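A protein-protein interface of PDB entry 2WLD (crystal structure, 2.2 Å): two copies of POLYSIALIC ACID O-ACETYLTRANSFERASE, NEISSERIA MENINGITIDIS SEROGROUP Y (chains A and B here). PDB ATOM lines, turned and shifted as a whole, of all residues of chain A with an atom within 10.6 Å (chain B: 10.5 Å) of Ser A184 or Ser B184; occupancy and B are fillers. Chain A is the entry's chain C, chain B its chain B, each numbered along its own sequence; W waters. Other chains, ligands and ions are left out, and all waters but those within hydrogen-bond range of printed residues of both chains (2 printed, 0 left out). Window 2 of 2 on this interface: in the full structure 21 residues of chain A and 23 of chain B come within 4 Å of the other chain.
A ring nitrogen (NE2) of His B167 is in hydrogen-bond range of the side-chain hydroxyl (OG1) of Thr A151 (3.0 Å).
Of the printed residues of chain B, Tyr A171 touches Gly B165 (3.8 Å), Ser B166 (3.9 Å) and Ala B182 (3.9 Å).
No residue of chain B comes within 4 Å of Gly A183.
Ser A184 touches one residue of chain B.
No residue of chain B comes within 4 Å of Pro A185.
Printed residues of chain A within 4 Å of Gly B165: Tyr A171.
Tyr B171 touches none of the printed residues of chain A.
No residue of chain A comes within 4 Å of Gly B183.
Of chain A, only Ser A184 comes within 4 Å of Ser B184.
No residue of chain A comes within 4 Å of Pro B185.
No residue of chain A comes within 4 Å of Ala B186.
The nearest residue of chain B that does not touch Ser A184 is Gly B183 (4.9 Å).
The nearest residue of chain A that does not touch Ser B184 is Pro A185 (4.5 Å).
Val A169 touches His B167, but with the chains exchanged His A167 does not touch Val B169 (9.7 Å).
Tyr A171 touches Ser B166, but with the chains exchanged Ser A166 does not touch Tyr B171 (16.2 Å).
Tyr A171 touches Ala B182, but with the chains exchanged Ala A182 does not touch Tyr B171 (17.3 Å).
Ser A184 touches its own counterpart, Ser B184.
Of the 6 pairs that touch across the chains among the printed residues, 1 has its exchanged pair printed and touching as well.
His B167 touches Val A169.
Tyr A171 touches Gly B165 (OH to CA, 3.8 Å).
N of Ser B166 touches OH of Tyr A171, 3.9 Å away.
Tyr A171 touches Ala B182.
Ser B184 touches Ser A184 (CB to OG, 3.3 Å).
N of Thr A151 lies within hydrogen-bond range of O of Thr A168 (3.0 Å).
The backbone NH (N) of Leu A170 sits at hydrogen-bond distance from the backbone carbonyl oxygen (O) of Thr A151, 2.9 Å away.
O of Ala B182 is in hydrogen-bond range of N of Lys B187 (2.9 Å).
The backbone NH of Gly B165 lies within hydrogen-bond range of the backbone carbonyl oxygen of Ile B181, at 2.7 Å.
Water W2 lies within hydrogen-bond range of the backbone carbonyl oxygen of Ser B184 (2.5 Å) and the backbone carbonyl oxygen of Ser A184 (2.7 Å).
Water W1 lies within hydrogen-bond range of O of His A167 and ND1 of His B167.
Hydrophobic or aromatic side chains of chain B within 4 Å of the printed part of chain A: His B167 and Ala B182.
Hydrophobic or aromatic side chains of chain A within 4 Å of the printed part of chain B: Val A169 and Tyr A171.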
ATOM      1  N   ASN A 149      -1.154 -12.505 -24.671  1.00  0.00           N
ATOM      2  CA  ASN A 149      -2.036 -11.829 -23.736  1.00  0.00           C
ATOM      3  C   ASN A 149      -3.475 -12.255 -23.863  1.00  0.00           C
ATOM      4  O   ASN A 149      -4.357 -11.416 -23.921  1.00  0.00           O
ATOM      5  CB  ASN A 149      -1.942 -10.312 -23.921  1.00  0.00           C
ATOM      6  CG  ASN A 149      -0.533  -9.795 -23.700  1.00  0.00           C
ATOM      7  OD1 ASN A 149       0.147  -9.336 -24.629  1.00  0.00           O
ATOM      8  ND2 ASN A 149      -0.085  -9.884 -22.487  1.00  0.00           N
ATOM      9  N   THR A 151      -6.781 -14.233 -22.274  1.00  0.00           N
ATOM     10  CA  THR A 151      -7.376 -14.488 -20.983  1.00  0.00           C
ATOM     11  C   THR A 151      -8.467 -15.531 -21.157  1.00  0.00           C
ATOM     12  O   THR A 151      -9.374 -15.375 -21.983  1.00  0.00           O
ATOM     13  CB  THR A 151      -8.003 -13.217 -20.393  1.00  0.00           C
ATOM     14  OG1 THR A 151      -6.989 -12.238 -20.164  1.00  0.00           O
ATOM     15  CG2 THR A 151      -8.712 -13.517 -19.057  1.00  0.00           C
ATOM     16  N   VAL A 164      -6.468 -18.847 -30.886  1.00  0.00           N
ATOM     17  CA  VAL A 164      -7.098 -17.685 -30.268  1.00  0.00           C
ATOM     18  C   VAL A 164      -6.245 -16.443 -30.479  1.00  0.00           C
ATOM     19  O   VAL A 164      -5.088 -16.404 -30.091  1.00  0.00           O
ATOM     20  CB  VAL A 164      -7.296 -17.902 -28.743  1.00  0.00           C
ATOM     21  CG1 VAL A 164      -7.957 -16.667 -28.097  1.00  0.00           C
ATOM     22  CG2 VAL A 164      -8.117 -19.126 -28.485  1.00  0.00           C
ATOM     23  N   GLY A 165      -6.825 -15.419 -31.091  1.00  0.00           N
ATOM     24  CA  GLY A 165      -6.106 -14.223 -31.452  1.00  0.00           C
ATOM     25  C   GLY A 165      -5.639 -13.442 -30.245  1.00  0.00           C
ATOM     26  O   GLY A 165      -6.279 -13.426 -29.186  1.00  0.00           O
ATOM     27  N   SER A 166      -4.514 -12.768 -30.422  1.00  0.00           N
ATOM     28  CA  SER A 166      -3.865 -12.062 -29.342  1.00  0.00           C
ATOM     29  C   SER A 166      -4.789 -11.005 -28.675  1.00  0.00           C
ATOM     30  O   SER A 166      -5.602 -10.377 -29.334  1.00  0.00           O
ATOM     31  CB  SER A 166      -2.544 -11.448 -29.873  1.00  0.00           C
ATOM     32  OG  SER A 166      -2.722 -10.112 -30.249  1.00  0.00           O
ATOM     33  N   HIS A 167      -4.650 -10.858 -27.357  1.00  0.00           N
ATOM     34  CA  HIS A 167      -5.463  -9.978 -26.507  1.00  0.00           C
ATOM     35  C   HIS A 167      -6.963 -10.324 -26.416  1.00  0.00           C
ATOM     36  O   HIS A 167      -7.759  -9.512 -25.974  1.00  0.00           O
ATOM     37  CB  HIS A 167      -5.323  -8.532 -26.942  1.00  0.00           C
ATOM     38  CG  HIS A 167      -3.919  -8.021 -26.887  1.00  0.00           C
ATOM     39  ND1 HIS A 167      -3.422  -7.323 -25.805  1.00  0.00           N
ATOM     40  CD2 HIS A 167      -2.914  -8.089 -27.796  1.00  0.00           C
ATOM     41  CE1 HIS A 167      -2.168  -6.984 -26.050  1.00  0.00           C
ATOM     42  NE2 HIS A 167      -1.838  -7.438 -27.253  1.00  0.00           N
ATOM     43  N   THR A 168      -7.344 -11.519 -26.828  1.00  0.00           N
ATOM     44  CA  THR A 168      -8.735 -11.957 -26.720  1.00  0.00           C
ATOM     45  C   THR A 168      -9.041 -12.502 -25.334  1.00  0.00           C
ATOM     46  O   THR A 168      -8.233 -13.237 -24.749  1.00  0.00           O
ATOM     47  CB  THR A 168      -8.994 -13.058 -27.721  1.00  0.00           C
ATOM     48  OG1 THR A 168      -8.604 -12.582 -29.024  1.00  0.00           O
ATOM     49  CG2 THR A 168     -10.497 -13.484 -27.705  1.00  0.00           C
ATOM     50  N   VAL A 169     -10.206 -12.109 -24.813  1.00  0.00           N
ATOM     51  CA  VAL A 169     -10.758 -12.640 -23.595  1.00  0.00           C
ATOM     52  C   VAL A 169     -11.879 -13.639 -23.938  1.00  0.00           C
ATOM     53  O   VAL A 169     -12.820 -13.282 -24.644  1.00  0.00           O
ATOM     54  CB  VAL A 169     -11.370 -11.495 -22.777  1.00  0.00           C
ATOM     55  CG1 VAL A 169     -11.985 -12.013 -21.486  1.00  0.00           C
ATOM     56  CG2 VAL A 169     -10.324 -10.456 -22.487  1.00  0.00           C
ATOM     57  N   LEU A 170     -11.776 -14.880 -23.465  1.00  0.00           N
ATOM     58  CA  LEU A 170     -12.877 -15.848 -23.626  1.00  0.00           C
ATOM     59  C   LEU A 170     -13.699 -15.966 -22.324  1.00  0.00           C
ATOM     60  O   LEU A 170     -13.144 -16.300 -21.276  1.00  0.00           O
ATOM     61  CB  LEU A 170     -12.359 -17.243 -24.033  1.00  0.00           C
ATOM     62  CG  LEU A 170     -11.518 -17.365 -25.311  1.00  0.00           C
ATOM     63  CD1 LEU A 170     -11.409 -18.847 -25.782  1.00  0.00           C
ATOM     64  CD2 LEU A 170     -12.107 -16.524 -26.391  1.00  0.00           C
ATOM     65  N   TYR A 171     -14.995 -15.674 -22.403  1.00  0.00           N
ATOM     66  CA  TYR A 171     -15.896 -15.756 -21.267  1.00  0.00           C
ATOM     67  C   TYR A 171     -16.757 -17.013 -21.375  1.00  0.00           C
ATOM     68  O   TYR A 171     -17.302 -17.469 -20.363  1.00  0.00           O
ATOM     69  CB  TYR A 171     -16.879 -14.577 -21.252  1.00  0.00           C
ATOM     70  CG  TYR A 171     -16.528 -13.417 -20.361  1.00  0.00           C
ATOM     71  CD1 TYR A 171     -16.893 -13.413 -19.017  1.00  0.00           C
ATOM     72  CD2 TYR A 171     -15.880 -12.279 -20.874  1.00  0.00           C
ATOM     73  CE1 TYR A 171     -16.599 -12.332 -18.187  1.00  0.00           C
ATOM     74  CE2 TYR A 171     -15.575 -11.193 -20.058  1.00  0.00           C
ATOM     75  CZ  TYR A 171     -15.938 -11.228 -18.713  1.00  0.00           C
ATOM     76  OH  TYR A 171     -15.644 -10.165 -17.888  1.00  0.00           O
ATOM     77  N   PHE A 174     -16.720 -22.559 -26.847  1.00  0.00           N
ATOM     78  CA  PHE A 174     -16.987 -22.749 -28.278  1.00  0.00           C
ATOM     79  C   PHE A 174     -17.005 -24.256 -28.566  1.00  0.00           C
ATOM     80  O   PHE A 174     -16.436 -25.037 -27.805  1.00  0.00           O
ATOM     81  CB  PHE A 174     -15.895 -22.071 -29.135  1.00  0.00           C
ATOM     82  CG  PHE A 174     -15.922 -20.576 -29.063  1.00  0.00           C
ATOM     83  CD1 PHE A 174     -15.354 -19.913 -27.991  1.00  0.00           C
ATOM     84  CD2 PHE A 174     -16.556 -19.832 -30.038  1.00  0.00           C
ATOM     85  CE1 PHE A 174     -15.409 -18.513 -27.891  1.00  0.00           C
ATOM     86  CE2 PHE A 174     -16.606 -18.428 -29.956  1.00  0.00           C
ATOM     87  CZ  PHE A 174     -16.033 -17.774 -28.874  1.00  0.00           C
ATOM     88  N   ILE A 181     -10.388 -17.849 -33.301  1.00  0.00           N
ATOM     89  CA  ILE A 181     -11.286 -17.082 -32.468  1.00  0.00           C
ATOM     90  C   ILE A 181     -10.578 -15.799 -32.030  1.00  0.00           C
ATOM     91  O   ILE A 181      -9.470 -15.863 -31.530  1.00  0.00           O
ATOM     92  CB  ILE A 181     -11.661 -17.853 -31.209  1.00  0.00           C
ATOM     93  CG1 ILE A 181     -12.498 -19.098 -31.560  1.00  0.00           C
ATOM     94  CG2 ILE A 181     -12.509 -16.981 -30.341  1.00  0.00           C
ATOM     95  CD1 ILE A 181     -12.566 -20.152 -30.423  1.00  0.00           C
ATOM     96  N   ALA A 182     -11.216 -14.651 -32.194  1.00  0.00           N
ATOM     97  CA  ALA A 182     -10.582 -13.375 -31.873  1.00  0.00           C
ATOM     98  C   ALA A 182     -11.633 -12.335 -31.697  1.00  0.00           C
ATOM     99  O   ALA A 182     -12.786 -12.556 -32.022  1.00  0.00           O
ATOM    100  CB  ALA A 182      -9.658 -12.950 -32.979  1.00  0.00           C
ATOM    101  N   GLY A 183     -11.232 -11.201 -31.148  1.00  0.00           N
ATOM    102  CA  GLY A 183     -12.119 -10.055 -31.043  1.00  0.00           C
ATOM    103  C   GLY A 183     -12.751  -9.873 -29.669  1.00  0.00           C
ATOM    104  O   GLY A 183     -12.498 -10.628 -28.717  1.00  0.00           O
ATOM    105  N   SER A 184     -13.592  -8.854 -29.586  1.00  0.00           N
ATOM    106  CA  SER A 184     -14.236  -8.482 -28.346  1.00  0.00           C
ATOM    107  C   SER A 184     -15.583  -7.922 -28.704  1.00  0.00           C
ATOM    108  O   SER A 184     -15.691  -6.763 -29.100  1.00  0.00           O
ATOM    109  CB  SER A 184     -13.414  -7.437 -27.621  1.00  0.00           C
ATOM    110  OG  SER A 184     -14.115  -6.989 -26.480  1.00  0.00           O
ATOM    111  N   PRO A 185     -16.619  -8.752 -28.572  1.00  0.00           N
ATOM    112  CA  PRO A 185     -16.420 -10.049 -27.952  1.00  0.00           C
ATOM    113  C   PRO A 185     -15.887 -11.157 -28.869  1.00  0.00           C
ATOM    114  O   PRO A 185     -15.930 -11.061 -30.097  1.00  0.00           O
ATOM    115  CB  PRO A 185     -17.810 -10.396 -27.413  1.00  0.00           C
ATOM    116  CG  PRO A 185     -18.771  -9.576 -28.194  1.00  0.00           C
ATOM    117  CD  PRO A 185     -18.026  -8.504 -28.924  1.00  0.00           C
ATOM    118  N   ALA A 186     -15.379 -12.199 -28.234  1.00  0.00           N
ATOM    119  CA  ALA A 186     -14.718 -13.290 -28.903  1.00  0.00           C
ATOM    120  C   ALA A 186     -15.658 -13.979 -29.908  1.00  0.00           C
ATOM    121  O   ALA A 186     -16.702 -14.512 -29.538  1.00  0.00           O
ATOM    122  CB  ALA A 186     -14.208 -14.297 -27.852  1.00  0.00           C
ATOM    123  N   LYS A 187     -15.300 -13.950 -31.185  1.00  0.00           N
ATOM    124  CA  LYS A 187     -16.070 -14.686 -32.175  1.00  0.00           C
ATOM    125  C   LYS A 187     -15.144 -15.425 -33.131  1.00  0.00           C
ATOM    126  O   LYS A 187     -13.951 -15.080 -33.271  1.00  0.00           O
ATOM    127  CB  LYS A 187     -17.020 -13.755 -32.935  1.00  0.00           C
ATOM    128  CG  LYS A 187     -16.346 -12.577 -33.638  1.00  0.00           C
ATOM    129  CD  LYS A 187     -17.369 -11.576 -34.197  1.00  0.00           C
ATOM    130  CE  LYS A 187     -18.162 -10.874 -33.097  1.00  0.00           C
ATOM    131  NZ  LYS A 187     -17.334  -9.974 -32.226  1.00  0.00           N
ATOM    132  N   ILE A 188     -15.686 -16.476 -33.749  1.00  0.00           N
ATOM    133  CA  ILE A 188     -14.987 -17.215 -34.772  1.00  0.00           C
ATOM    134  C   ILE A 188     -14.767 -16.273 -35.942  1.00  0.00           C
ATOM    135  O   ILE A 188     -15.713 -15.677 -36.415  1.00  0.00           O
ATOM    136  CB  ILE A 188     -15.794 -18.429 -35.203  1.00  0.00           C
ATOM    137  CG1 ILE A 188     -15.879 -19.408 -34.028  1.00  0.00           C
ATOM    138  CG2 ILE A 188     -15.139 -19.129 -36.432  1.00  0.00           C
ATOM    139  CD1 ILE A 188     -16.813 -20.570 -34.267  1.00  0.00           C
ATOM    140  N   VAL A 189     -13.532 -16.119 -36.404  1.00  0.00           N
ATOM    141  CA  VAL A 189     -13.260 -15.171 -37.487  1.00  0.00           C
ATOM    142  C   VAL A 189     -12.708 -15.874 -38.709  1.00  0.00           C
ATOM    143  O   VAL A 189     -12.601 -15.297 -39.774  1.00  0.00           O
ATOM    144  CB  VAL A 189     -12.252 -14.053 -37.072  1.00  0.00           C
ATOM    145  CG1 VAL A 189     -12.900 -13.037 -36.119  1.00  0.00           C
ATOM    146  CG2 VAL A 189     -10.976 -14.671 -36.480  1.00  0.00           C
ATOM    147  N   THR B 151      -9.283  -0.472 -17.542  1.00  0.00           N
ATOM    148  CA  THR B 151      -8.842   0.870 -17.875  1.00  0.00           C
ATOM    149  C   THR B 151      -9.985   1.853 -17.684  1.00  0.00           C
ATOM    150  O   THR B 151     -11.070   1.694 -18.265  1.00  0.00           O
ATOM    151  CB  THR B 151      -8.353   0.952 -19.322  1.00  0.00           C
ATOM    152  OG1 THR B 151      -7.133   0.219 -19.463  1.00  0.00           O
ATOM    153  CG2 THR B 151      -8.103   2.397 -19.701  1.00  0.00           C
ATOM    154  N   VAL B 164     -16.421  -4.255 -12.337  1.00  0.00           N
ATOM    155  CA  VAL B 164     -16.042  -4.055 -13.728  1.00  0.00           C
ATOM    156  C   VAL B 164     -15.242  -5.272 -14.163  1.00  0.00           C
ATOM    157  O   VAL B 164     -14.237  -5.631 -13.542  1.00  0.00           O
ATOM    158  CB  VAL B 164     -15.231  -2.765 -13.929  1.00  0.00           C
ATOM    159  CG1 VAL B 164     -14.867  -2.595 -15.387  1.00  0.00           C
ATOM    160  CG2 VAL B 164     -16.018  -1.534 -13.420  1.00  0.00           C
ATOM    161  N   GLY B 165     -15.734  -5.931 -15.211  1.00  0.00           N
ATOM    162  CA  GLY B 165     -15.161  -7.174 -15.673  1.00  0.00           C
ATOM    163  C   GLY B 165     -13.779  -6.987 -16.258  1.00  0.00           C
ATOM    164  O   GLY B 165     -13.466  -5.966 -16.877  1.00  0.00           O
ATOM    165  N   SER B 166     -12.967  -8.018 -16.070  1.00  0.00           N
ATOM    166  CA  SER B 166     -11.586  -8.062 -16.514  1.00  0.00           C
ATOM    167  C   SER B 166     -11.390  -7.560 -17.948  1.00  0.00           C
ATOM    168  O   SER B 166     -12.168  -7.884 -18.849  1.00  0.00           O
ATOM    169  CB  SER B 166     -11.076  -9.504 -16.362  1.00  0.00           C
ATOM    170  OG  SER B 166      -9.976  -9.768 -17.216  1.00  0.00           O
ATOM    171  N   HIS B 167     -10.340  -6.757 -18.125  1.00  0.00           N
ATOM    172  CA  HIS B 167      -9.920  -6.190 -19.421  1.00  0.00           C
ATOM    173  C   HIS B 167     -10.925  -5.229 -20.044  1.00  0.00           C
ATOM    174  O   HIS B 167     -10.750  -4.840 -21.189  1.00  0.00           O
ATOM    175  CB  HIS B 167      -9.539  -7.293 -20.436  1.00  0.00           C
ATOM    176  CG  HIS B 167      -8.317  -8.066 -20.044  1.00  0.00           C
ATOM    177  ND1 HIS B 167      -7.075  -7.846 -20.610  1.00  0.00           N
ATOM    178  CD2 HIS B 167      -8.140  -9.037 -19.116  1.00  0.00           C
ATOM    179  CE1 HIS B 167      -6.193  -8.652 -20.048  1.00  0.00           C
ATOM    180  NE2 HIS B 167      -6.811  -9.375 -19.129  1.00  0.00           N
ATOM    181  N   THR B 168     -11.962  -4.842 -19.302  1.00  0.00           N
ATOM    182  CA  THR B 168     -12.892  -3.830 -19.795  1.00  0.00           C
ATOM    183  C   THR B 168     -12.267  -2.425 -19.818  1.00  0.00           C
ATOM    184  O   THR B 168     -11.562  -2.018 -18.887  1.00  0.00           O
ATOM    185  CB  THR B 168     -14.144  -3.728 -18.926  1.00  0.00           C
ATOM    186  OG1 THR B 168     -14.699  -5.030 -18.665  1.00  0.00           O
ATOM    187  CG2 THR B 168     -15.174  -2.856 -19.621  1.00  0.00           C
ATOM    188  N   VAL B 169     -12.560  -1.682 -20.876  1.00  0.00           N
ATOM    189  CA  VAL B 169     -12.155  -0.291 -20.996  1.00  0.00           C
ATOM    190  C   VAL B 169     -13.369   0.623 -20.797  1.00  0.00           C
ATOM    191  O   VAL B 169     -14.344   0.528 -21.539  1.00  0.00           O
ATOM    192  CB  VAL B 169     -11.547  -0.039 -22.386  1.00  0.00           C
ATOM    193  CG1 VAL B 169     -11.354   1.463 -22.655  1.00  0.00           C
ATOM    194  CG2 VAL B 169     -10.236  -0.757 -22.501  1.00  0.00           C
ATOM    195  N   LEU B 170     -13.327   1.498 -19.802  1.00  0.00           N
ATOM    196  CA  LEU B 170     -14.416   2.453 -19.629  1.00  0.00           C
ATOM    197  C   LEU B 170     -14.100   3.859 -20.189  1.00  0.00           C
ATOM    198  O   LEU B 170     -13.126   4.499 -19.796  1.00  0.00           O
ATOM    199  CB  LEU B 170     -14.820   2.564 -18.148  1.00  0.00           C
ATOM    200  CG  LEU B 170     -15.847   1.564 -17.600  1.00  0.00           C
ATOM    201  CD1 LEU B 170     -15.306   0.169 -17.570  1.00  0.00           C
ATOM    202  CD2 LEU B 170     -16.318   1.982 -16.179  1.00  0.00           C
ATOM    203  N   TYR B 171     -14.969   4.303 -21.097  1.00  0.00           N
ATOM    204  CA  TYR B 171     -14.923   5.619 -21.748  1.00  0.00           C
ATOM    205  C   TYR B 171     -16.012   6.545 -21.184  1.00  0.00           C
ATOM    206  O   TYR B 171     -15.894   7.764 -21.246  1.00  0.00           O
ATOM    207  CB  TYR B 171     -15.195   5.480 -23.257  1.00  0.00           C
ATOM    208  CG  TYR B 171     -13.977   5.261 -24.122  1.00  0.00           C
ATOM    209  CD1 TYR B 171     -13.185   6.334 -24.508  1.00  0.00           C
ATOM    210  CD2 TYR B 171     -13.630   3.987 -24.593  1.00  0.00           C
ATOM    211  CE1 TYR B 171     -12.063   6.151 -25.305  1.00  0.00           C
ATOM    212  CE2 TYR B 171     -12.495   3.798 -25.409  1.00  0.00           C
ATOM    213  CZ  TYR B 171     -11.725   4.893 -25.748  1.00  0.00           C
ATOM    214  OH  TYR B 171     -10.596   4.772 -26.539  1.00  0.00           O
ATOM    215  N   PHE B 174     -21.489   5.518 -15.938  1.00  0.00           N
ATOM    216  CA  PHE B 174     -22.742   4.807 -15.728  1.00  0.00           C
ATOM    217  C   PHE B 174     -23.439   5.413 -14.504  1.00  0.00           C
ATOM    218  O   PHE B 174     -22.797   6.097 -13.705  1.00  0.00           O
ATOM    219  CB  PHE B 174     -22.464   3.323 -15.508  1.00  0.00           C
ATOM    220  CG  PHE B 174     -21.971   2.616 -16.729  1.00  0.00           C
ATOM    221  CD1 PHE B 174     -20.630   2.659 -17.080  1.00  0.00           C
ATOM    222  CD2 PHE B 174     -22.841   1.898 -17.528  1.00  0.00           C
ATOM    223  CE1 PHE B 174     -20.178   1.996 -18.206  1.00  0.00           C
ATOM    224  CE2 PHE B 174     -22.383   1.235 -18.666  1.00  0.00           C
ATOM    225  CZ  PHE B 174     -21.064   1.284 -18.998  1.00  0.00           C
ATOM    226  N   ILE B 181     -20.350  -4.558 -15.007  1.00  0.00           N
ATOM    227  CA  ILE B 181     -20.134  -3.918 -16.280  1.00  0.00           C
ATOM    228  C   ILE B 181     -18.950  -4.579 -16.940  1.00  0.00           C
ATOM    229  O   ILE B 181     -17.907  -4.738 -16.311  1.00  0.00           O
ATOM    230  CB  ILE B 181     -19.827  -2.440 -16.111  1.00  0.00           C
ATOM    231  CG1 ILE B 181     -21.033  -1.715 -15.526  1.00  0.00           C
ATOM    232  CG2 ILE B 181     -19.445  -1.816 -17.438  1.00  0.00           C
ATOM    233  CD1 ILE B 181     -20.724  -0.249 -15.148  1.00  0.00           C
ATOM    234  N   ALA B 182     -19.125  -4.982 -18.193  1.00  0.00           N
ATOM    235  CA  ALA B 182     -18.062  -5.610 -18.963  1.00  0.00           C
ATOM    236  C   ALA B 182     -18.345  -5.395 -20.438  1.00  0.00           C
ATOM    237  O   ALA B 182     -19.336  -4.765 -20.789  1.00  0.00           O
ATOM    238  CB  ALA B 182     -17.991  -7.102 -18.660  1.00  0.00           C
ATOM    239  N   GLY B 183     -17.483  -5.935 -21.296  1.00  0.00           N
ATOM    240  CA  GLY B 183     -17.679  -5.828 -22.737  1.00  0.00           C
ATOM    241  C   GLY B 183     -17.061  -4.582 -23.353  1.00  0.00           C
ATOM    242  O   GLY B 183     -16.550  -3.677 -22.665  1.00  0.00           O
ATOM    243  N   SER B 184     -17.131  -4.552 -24.667  1.00  0.00           N
ATOM    244  CA  SER B 184     -16.600  -3.487 -25.472  1.00  0.00           C
ATOM    245  C   SER B 184     -17.582  -3.337 -26.608  1.00  0.00           C
ATOM    246  O   SER B 184     -17.778  -4.258 -27.368  1.00  0.00           O
ATOM    247  CB  SER B 184     -15.231  -3.891 -26.022  1.00  0.00           C
ATOM    248  OG  SER B 184     -14.869  -3.074 -27.116  1.00  0.00           O
ATOM    249  N   PRO B 185     -18.274  -2.202 -26.676  1.00  0.00           N
ATOM    250  CA  PRO B 185     -18.226  -1.117 -25.694  1.00  0.00           C
ATOM    251  C   PRO B 185     -18.730  -1.557 -24.324  1.00  0.00           C
ATOM    252  O   PRO B 185     -19.559  -2.445 -24.226  1.00  0.00           O
ATOM    253  CB  PRO B 185     -19.140  -0.036 -26.288  1.00  0.00           C
ATOM    254  CG  PRO B 185     -19.450  -0.484 -27.711  1.00  0.00           C
ATOM    255  CD  PRO B 185     -19.233  -1.956 -27.766  1.00  0.00           C
ATOM    256  N   ALA B 186     -18.209  -0.935 -23.278  1.00  0.00           N
ATOM    257  CA  ALA B 186     -18.550  -1.305 -21.917  1.00  0.00           C
ATOM    258  C   ALA B 186     -20.057  -1.244 -21.702  1.00  0.00           C
ATOM    259  O   ALA B 186     -20.722  -0.338 -22.184  1.00  0.00           O
ATOM    260  CB  ALA B 186     -17.836  -0.391 -20.940  1.00  0.00           C
ATOM    261  N   LYS B 187     -20.596  -2.207 -20.971  1.00  0.00           N
ATOM    262  CA  LYS B 187     -22.043  -2.307 -20.828  1.00  0.00           C
ATOM    263  C   LYS B 187     -22.429  -2.959 -19.525  1.00  0.00           C
ATOM    264  O   LYS B 187     -21.677  -3.784 -19.007  1.00  0.00           O
ATOM    265  CB  LYS B 187     -22.593  -3.148 -21.964  1.00  0.00           C
ATOM    266  CG  LYS B 187     -23.943  -2.742 -22.410  1.00  0.00           C
ATOM    267  CD  LYS B 187     -24.144  -3.170 -23.841  1.00  0.00           C
ATOM    268  CE  LYS B 187     -25.611  -3.452 -24.132  1.00  0.00           C
ATOM    269  NZ  LYS B 187     -25.772  -4.432 -25.249  1.00  0.00           N
ATOM    270  N   ILE B 188     -23.606  -2.599 -18.999  1.00  0.00           N
ATOM    271  CA  ILE B 188     -24.186  -3.312 -17.861  1.00  0.00           C
ATOM    272  C   ILE B 188     -24.573  -4.701 -18.347  1.00  0.00           C
ATOM    273  O   ILE B 188     -25.341  -4.836 -19.302  1.00  0.00           O
ATOM    274  CB  ILE B 188     -25.458  -2.614 -17.296  1.00  0.00           C
ATOM    275  CG1 ILE B 188     -25.103  -1.302 -16.594  1.00  0.00           C
ATOM    276  CG2 ILE B 188     -26.187  -3.528 -16.310  1.00  0.00           C
ATOM    277  CD1 ILE B 188     -26.309  -0.488 -16.168  1.00  0.00           C
ATOM    278  N   VAL B 189     -24.041  -5.735 -17.707  1.00  0.00           N
ATOM    279  CA  VAL B 189     -24.305  -7.087 -18.158  1.00  0.00           C
ATOM    280  C   VAL B 189     -25.021  -7.884 -17.105  1.00  0.00           C
ATOM    281  O   VAL B 189     -25.527  -8.944 -17.403  1.00  0.00           O
ATOM    282  CB  VAL B 189     -23.019  -7.830 -18.524  1.00  0.00           C
ATOM    283  CG1 VAL B 189     -22.390  -7.210 -19.776  1.00  0.00           C
ATOM    284  CG2 VAL B 189     -22.038  -7.834 -17.352  1.00  0.00           C
HETATM  285  O   HOH W   1      -7.219  -8.181 -23.732  1.00  0.00           O
HETATM  286  O   HOH W   2     -17.449  -4.776 -29.819  1.00  0.00           O
